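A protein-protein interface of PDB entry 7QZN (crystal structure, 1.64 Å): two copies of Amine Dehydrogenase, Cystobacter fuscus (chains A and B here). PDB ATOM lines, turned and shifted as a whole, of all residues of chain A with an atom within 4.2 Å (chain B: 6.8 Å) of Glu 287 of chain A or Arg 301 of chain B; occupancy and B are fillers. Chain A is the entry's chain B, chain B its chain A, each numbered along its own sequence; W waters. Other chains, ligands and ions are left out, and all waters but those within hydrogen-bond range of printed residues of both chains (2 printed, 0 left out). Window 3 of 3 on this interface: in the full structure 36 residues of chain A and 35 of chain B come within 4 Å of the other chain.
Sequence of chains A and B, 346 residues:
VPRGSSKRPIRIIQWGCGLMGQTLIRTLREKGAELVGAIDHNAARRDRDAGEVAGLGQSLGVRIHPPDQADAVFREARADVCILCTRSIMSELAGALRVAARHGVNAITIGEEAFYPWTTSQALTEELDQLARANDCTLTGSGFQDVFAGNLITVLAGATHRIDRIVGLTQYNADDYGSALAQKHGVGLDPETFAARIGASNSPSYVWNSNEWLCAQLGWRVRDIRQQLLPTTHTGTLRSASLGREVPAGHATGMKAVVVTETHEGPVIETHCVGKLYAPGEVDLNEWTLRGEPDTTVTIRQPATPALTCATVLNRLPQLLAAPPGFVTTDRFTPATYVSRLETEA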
ATOM      1  N   VAL A 167      23.482  13.850  25.314  1.00  0.00           N
ATOM      2  CA  VAL A 167      24.399  13.944  24.157  1.00  0.00           C
ATOM      3  C   VAL A 167      23.708  14.717  23.051  1.00  0.00           C
ATOM      4  O   VAL A 167      22.610  14.329  22.636  1.00  0.00           O
ATOM      5  CB  VAL A 167      24.827  12.545  23.674  1.00  0.00           C
ATOM      6  CG1 VAL A 167      25.715  12.620  22.463  1.00  0.00           C
ATOM      7  CG2 VAL A 167      25.489  11.798  24.830  1.00  0.00           C
ATOM      8  N   GLY A 168      24.355  15.770  22.591  1.00  0.00           N
ATOM      9  CA  GLY A 168      23.826  16.668  21.553  1.00  0.00           C
ATOM     10  C   GLY A 168      24.697  16.789  20.334  1.00  0.00           C
ATOM     11  O   GLY A 168      25.944  16.675  20.428  1.00  0.00           O
ATOM     12  N   LEU A 169      24.059  17.010  19.187  1.00  0.00           N
ATOM     13  CA  LEU A 169      24.717  17.413  17.935  1.00  0.00           C
ATOM     14  C   LEU A 169      23.966  18.618  17.388  1.00  0.00           C
ATOM     15  O   LEU A 169      22.738  18.561  17.173  1.00  0.00           O
ATOM     16  CB  LEU A 169      24.718  16.253  16.934  1.00  0.00           C
ATOM     17  CG  LEU A 169      25.222  16.647  15.552  1.00  0.00           C
ATOM     18  CD1 LEU A 169      26.696  16.968  15.583  1.00  0.00           C
ATOM     19  CD2 LEU A 169      24.932  15.547  14.534  1.00  0.00           C
ATOM     20  N   ASN A 286      20.121  18.997  14.163  1.00  0.00           N
ATOM     21  CA  ASN A 286      19.874  19.165  15.615  1.00  0.00           C
ATOM     22  C   ASN A 286      19.330  17.843  16.117  1.00  0.00           C
ATOM     23  O   ASN A 286      18.240  17.419  15.696  1.00  0.00           O
ATOM     24  CB  ASN A 286      18.980  20.359  15.903  1.00  0.00           C
ATOM     25  CG  ASN A 286      18.973  20.754  17.369  1.00  0.00           C
ATOM     26  OD1 ASN A 286      19.647  21.713  17.777  1.00  0.00           O
ATOM     27  ND2 ASN A 286      18.259  19.988  18.148  1.00  0.00           N
ATOM     28  N   GLU A 287      20.094  17.186  16.966  1.00  0.00           N
ATOM     29  CA  GLU A 287      19.700  15.880  17.492  1.00  0.00           C
ATOM     30  C   GLU A 287      20.260  15.734  18.909  1.00  0.00           C
ATOM     31  O   GLU A 287      21.450  15.999  19.143  1.00  0.00           O
ATOM     32  CB  GLU A 287      20.152  14.765  16.548  1.00  0.00           C
ATOM     33  CG  GLU A 287      19.742  13.407  17.011  1.00  0.00           C
ATOM     34  CD  GLU A 287      19.706  12.391  15.887  1.00  0.00           C
ATOM     35  OE1 GLU A 287      20.289  11.317  16.089  1.00  0.00           O
ATOM     36  OE2 GLU A 287      19.067  12.672  14.867  1.00  0.00           O
ATOM     37  N   TRP A 288      19.414  15.286  19.804  1.00  0.00           N
ATOM     38  CA  TRP A 288      19.732  15.121  21.231  1.00  0.00           C
ATOM     39  C   TRP A 288      19.271  13.777  21.724  1.00  0.00           C
ATOM     40  O   TRP A 288      18.170  13.354  21.356  1.00  0.00           O
ATOM     41  CB  TRP A 288      19.131  16.225  22.076  1.00  0.00           C
ATOM     42  CG  TRP A 288      19.660  17.579  21.767  1.00  0.00           C
ATOM     43  CD1 TRP A 288      19.245  18.423  20.793  1.00  0.00           C
ATOM     44  CD2 TRP A 288      20.726  18.258  22.455  1.00  0.00           C
ATOM     45  NE1 TRP A 288      20.020  19.536  20.777  1.00  0.00           N
ATOM     46  CE2 TRP A 288      20.902  19.500  21.817  1.00  0.00           C
ATOM     47  CE3 TRP A 288      21.507  17.960  23.579  1.00  0.00           C
ATOM     48  CZ2 TRP A 288      21.853  20.440  22.232  1.00  0.00           C
ATOM     49  CZ3 TRP A 288      22.470  18.864  23.963  1.00  0.00           C
ATOM     50  CH2 TRP A 288      22.654  20.079  23.289  1.00  0.00           C
ATOM     51  N   THR A 297      15.550  10.001  22.177  1.00  0.00           N
ATOM     52  CA  THR A 297      16.216  10.738  21.087  1.00  0.00           C
ATOM     53  C   THR A 297      15.204  11.644  20.404  1.00  0.00           C
ATOM     54  O   THR A 297      14.148  11.186  19.985  1.00  0.00           O
ATOM     55  CB  THR A 297      16.933   9.819  20.090  1.00  0.00           C
ATOM     56  OG1 THR A 297      17.891   9.046  20.807  1.00  0.00           O
ATOM     57  CG2 THR A 297      17.581  10.628  18.991  1.00  0.00           C
ATOM     58  N   VAL A 298      15.571  12.913  20.265  1.00  0.00           N
ATOM     59  CA  VAL A 298      14.792  13.946  19.536  1.00  0.00           C
ATOM     60  C   VAL A 298      15.611  14.447  18.356  1.00  0.00           C
ATOM     61  O   VAL A 298      16.828  14.709  18.488  1.00  0.00           O
ATOM     62  CB  VAL A 298      14.344  15.101  20.444  1.00  0.00           C
ATOM     63  CG1 VAL A 298      15.525  15.792  21.093  1.00  0.00           C
ATOM     64  CG2 VAL A 298      13.477  16.066  19.688  1.00  0.00           C
ATOM     65  N   THR A 299      14.939  14.608  17.223  1.00  0.00           N
ATOM     66  CA  THR A 299      15.572  15.112  15.981  1.00  0.00           C
ATOM     67  C   THR A 299      14.733  16.263  15.463  1.00  0.00           C
ATOM     68  O   THR A 299      13.501  16.100  15.396  1.00  0.00           O
ATOM     69  CB  THR A 299      15.665  14.015  14.911  1.00  0.00           C
ATOM     70  OG1 THR A 299      16.407  12.929  15.471  1.00  0.00           O
ATOM     71  CG2 THR A 299      16.357  14.549  13.673  1.00  0.00           C
ATOM     72  N   VAL B 283       6.285   0.550  15.452  1.00  0.00           N
ATOM     73  CA  VAL B 283       6.761   1.149  16.725  1.00  0.00           C
ATOM     74  C   VAL B 283       5.921   2.369  17.042  1.00  0.00           C
ATOM     75  O   VAL B 283       5.173   2.841  16.180  1.00  0.00           O
ATOM     76  CB  VAL B 283       8.236   1.550  16.610  1.00  0.00           C
ATOM     77  CG1 VAL B 283       9.093   0.286  16.564  1.00  0.00           C
ATOM     78  CG2 VAL B 283       8.507   2.505  15.458  1.00  0.00           C
ATOM     79  N   ASP B 284       6.034   2.842  18.281  1.00  0.00           N
ATOM     80  CA  ASP B 284       5.379   4.103  18.641  1.00  0.00           C
ATOM     81  C   ASP B 284       5.992   5.241  17.821  1.00  0.00           C
ATOM     82  O   ASP B 284       7.194   5.235  17.528  1.00  0.00           O
ATOM     83  CB  ASP B 284       5.570   4.387  20.140  1.00  0.00           C
ATOM     84  CG  ASP B 284       4.839   3.467  21.090  1.00  0.00           C
ATOM     85  OD1 ASP B 284       4.162   2.527  20.603  1.00  0.00           O
ATOM     86  OD2 ASP B 284       4.978   3.685  22.305  1.00  0.00           O
ATOM     87  N   ASN B 286       6.002   9.684  17.286  1.00  0.00           N
ATOM     88  CA  ASN B 286       5.664  11.043  17.775  1.00  0.00           C
ATOM     89  C   ASN B 286       6.351  12.015  16.861  1.00  0.00           C
ATOM     90  O   ASN B 286       7.588  12.048  16.832  1.00  0.00           O
ATOM     91  CB  ASN B 286       6.024  11.223  19.240  1.00  0.00           C
ATOM     92  CG  ASN B 286       5.370  12.447  19.854  1.00  0.00           C
ATOM     93  OD1 ASN B 286       4.317  12.357  20.506  1.00  0.00           O
ATOM     94  ND2 ASN B 286       5.938  13.583  19.546  1.00  0.00           N
ATOM     95  N   THR B 299      10.778  15.130  15.626  1.00  0.00           N
ATOM     96  CA  THR B 299      10.538  13.667  15.663  1.00  0.00           C
ATOM     97  C   THR B 299      11.128  13.137  16.963  1.00  0.00           C
ATOM     98  O   THR B 299      12.329  13.435  17.221  1.00  0.00           O
ATOM     99  CB  THR B 299      11.107  12.936  14.437  1.00  0.00           C
ATOM    100  OG1 THR B 299      10.557  13.624  13.300  1.00  0.00           O
ATOM    101  CG2 THR B 299      10.797  11.461  14.506  1.00  0.00           C
ATOM    102  N   ILE B 300      10.329  12.414  17.746  1.00  0.00           N
ATOM    103  CA  ILE B 300      10.887  11.537  18.818  1.00  0.00           C
ATOM    104  C   ILE B 300      11.069  10.153  18.196  1.00  0.00           C
ATOM    105  O   ILE B 300      10.106   9.589  17.696  1.00  0.00           O
ATOM    106  CB  ILE B 300      10.005  11.522  20.085  1.00  0.00           C
ATOM    107  CG1 ILE B 300       9.602  12.933  20.540  1.00  0.00           C
ATOM    108  CG2 ILE B 300      10.695  10.728  21.180  1.00  0.00           C
ATOM    109  CD1 ILE B 300      10.796  13.771  20.898  1.00  0.00           C
ATOM    110  N   ARG B 301      12.283   9.612  18.280  1.00  0.00           N
ATOM    111  CA  ARG B 301      12.609   8.309  17.665  1.00  0.00           C
ATOM    112  C   ARG B 301      12.143   7.220  18.627  1.00  0.00           C
ATOM    113  O   ARG B 301      12.790   7.082  19.668  1.00  0.00           O
ATOM    114  CB  ARG B 301      14.114   8.254  17.414  1.00  0.00           C
ATOM    115  CG  ARG B 301      14.666   9.327  16.487  1.00  0.00           C
ATOM    116  CD  ARG B 301      16.020   8.830  15.954  1.00  0.00           C
ATOM    117  NE  ARG B 301      16.736   9.800  15.131  1.00  0.00           N
ATOM    118  CZ  ARG B 301      16.418  10.126  13.883  1.00  0.00           C
ATOM    119  NH1 ARG B 301      15.365   9.578  13.294  1.00  0.00           N
ATOM    120  NH2 ARG B 301      17.158  11.010  13.228  1.00  0.00           N
ATOM    121  N   GLN B 302      11.051   6.526  18.338  1.00  0.00           N
ATOM    122  CA  GLN B 302      10.552   5.406  19.156  1.00  0.00           C
ATOM    123  C   GLN B 302      10.416   5.854  20.599  1.00  0.00           C
ATOM    124  O   GLN B 302      11.084   5.343  21.505  1.00  0.00           O
ATOM    125  CB  GLN B 302      11.474   4.190  19.044  1.00  0.00           C
ATOM    126  CG  GLN B 302      11.535   3.723  17.602  1.00  0.00           C
ATOM    127  CD  GLN B 302      12.344   2.459  17.420  1.00  0.00           C
ATOM    128  OE1 GLN B 302      12.107   1.489  18.129  1.00  0.00           O
ATOM    129  NE2 GLN B 302      13.352   2.526  16.548  1.00  0.00           N
ATOM    130  N   PRO B 303       9.500   6.789  20.882  1.00  0.00           N
ATOM    131  CA  PRO B 303       9.286   7.184  22.277  1.00  0.00           C
ATOM    132  C   PRO B 303       8.923   5.953  23.121  1.00  0.00           C
ATOM    133  O   PRO B 303       8.072   5.164  22.721  1.00  0.00           O
ATOM    134  CB  PRO B 303       8.097   8.134  22.238  1.00  0.00           C
ATOM    135  CG  PRO B 303       7.403   7.846  20.881  1.00  0.00           C
ATOM    136  CD  PRO B 303       8.536   7.408  19.957  1.00  0.00           C
ATOM    137  N   ALA B 304       9.523   5.842  24.316  1.00  0.00           N
ATOM    138  CA  ALA B 304       9.190   4.798  25.312  1.00  0.00           C
ATOM    139  C   ALA B 304       7.924   5.226  26.078  1.00  0.00           C
ATOM    140  O   ALA B 304       8.013   5.697  27.239  1.00  0.00           O
ATOM    141  CB  ALA B 304      10.382   4.603  26.220  1.00  0.00           C
HETATM  142  O   HOH W   1      13.247   8.108  22.021  1.00  0.00           O
HETATM  143  O   HOH W   2      12.368  15.410  12.698  1.00  0.00           O
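N of Thr 299 of chain A sits at hydrogen-bond distance from O of Thr 299 of chain B (2.9 Å).
The guanidinium group of Arg 301 of chain B lies within salt-bridge range of the side-chain carboxylate of Glu 287 of chain A.
The backbone NH of Arg 301 of chain B is in hydrogen-bond range of the backbone carbonyl oxygen of Thr 297 of chain A.
OG1 of Thr 299 of chain A is in hydrogen-bond range of NH2 of Arg 301 of chain B (3.0 Å).
The backbone carbonyl oxygen (O) of Asn 286 of chain B sits at hydrogen-bond distance from the backbone NH (N) of Ile 300 of chain B, at 2.9 Å.
The backbone carbonyl oxygen (O) of Glu 287 of chain A sits at hydrogen-bond distance from the backbone NH (N) of Leu 169 of chain A, at 2.8 Å.
OE2 of Glu 287 of chain A is in hydrogen-bond range of OG1 of Thr 299 of chain A, 2.7 Å away.
O of Trp 288 of chain A is in hydrogen-bond range of N of Val 298 of chain A.
Among the printed residues, pairs that only touch across the chains: Val 298 of chain A with Thr 299 of chain B (3.4 Å), Thr 297 of chain A with Ile 300 of chain B (3.5 Å) and Val 298 of chain A with Ile 300 of chain B (3.7 Å).
Of chain A, only Glu 287 (3.0 Å), Thr 297 (3.0 Å) and Thr 299 (3.0 Å) come within 4 Å of Arg 301 of chain B.
Printed residues of chain A within 4 Å of Ile 300 of chain B: Thr 297 (3.5 Å) and Val 298 (3.7 Å).
Of the printed residues of chain B, Val 298 of chain A touches Thr 299 (3.4 Å) and Ile 300 (3.7 Å).
Printed residues of chain B within 4 Å of Thr 299 of chain A: Thr 299 and Arg 301.
Of the printed residues of chain A, Thr 299 of chain B touches Val 298 and Thr 299.
The nearest printed residue of chain A that does not touch Arg 301 of chain B is Val 298 of chain A (5.1 Å).
The nearest printed residue of chain B that does not touch Thr 297 of chain A is Thr 299 of chain B (4.001 Å).
Along chain B the printed residues that touch a printed residue of chain A span positions 299 to 301.
Among the printed residues, Asp or Glu carboxylates within 4 Å of a Lys or Arg side-chain nitrogen of the other chain: Glu 287 of chain A with Arg 301 of chain B.
Thr 299 of chain A touches its own counterpart, Thr 299 of chain B.
Positions printed for both chains: 286 and 299.
Of the 7 pairs that touch across the chains among the printed residues, 1 has its exchanged pair printed and touching as well.
Water W1 lies within hydrogen-bond range of the backbone carbonyl oxygen (O) of Arg 301 of chain B (2.6 Å) and the backbone NH (N) of Thr 297 of chain A (3.0 Å).
Water W2 lies within hydrogen-bond range of the side-chain hydroxyl of Thr 299 of chain B (2.6 Å) and the backbone carbonyl oxygen of Thr 299 of chain A (3.0 Å).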
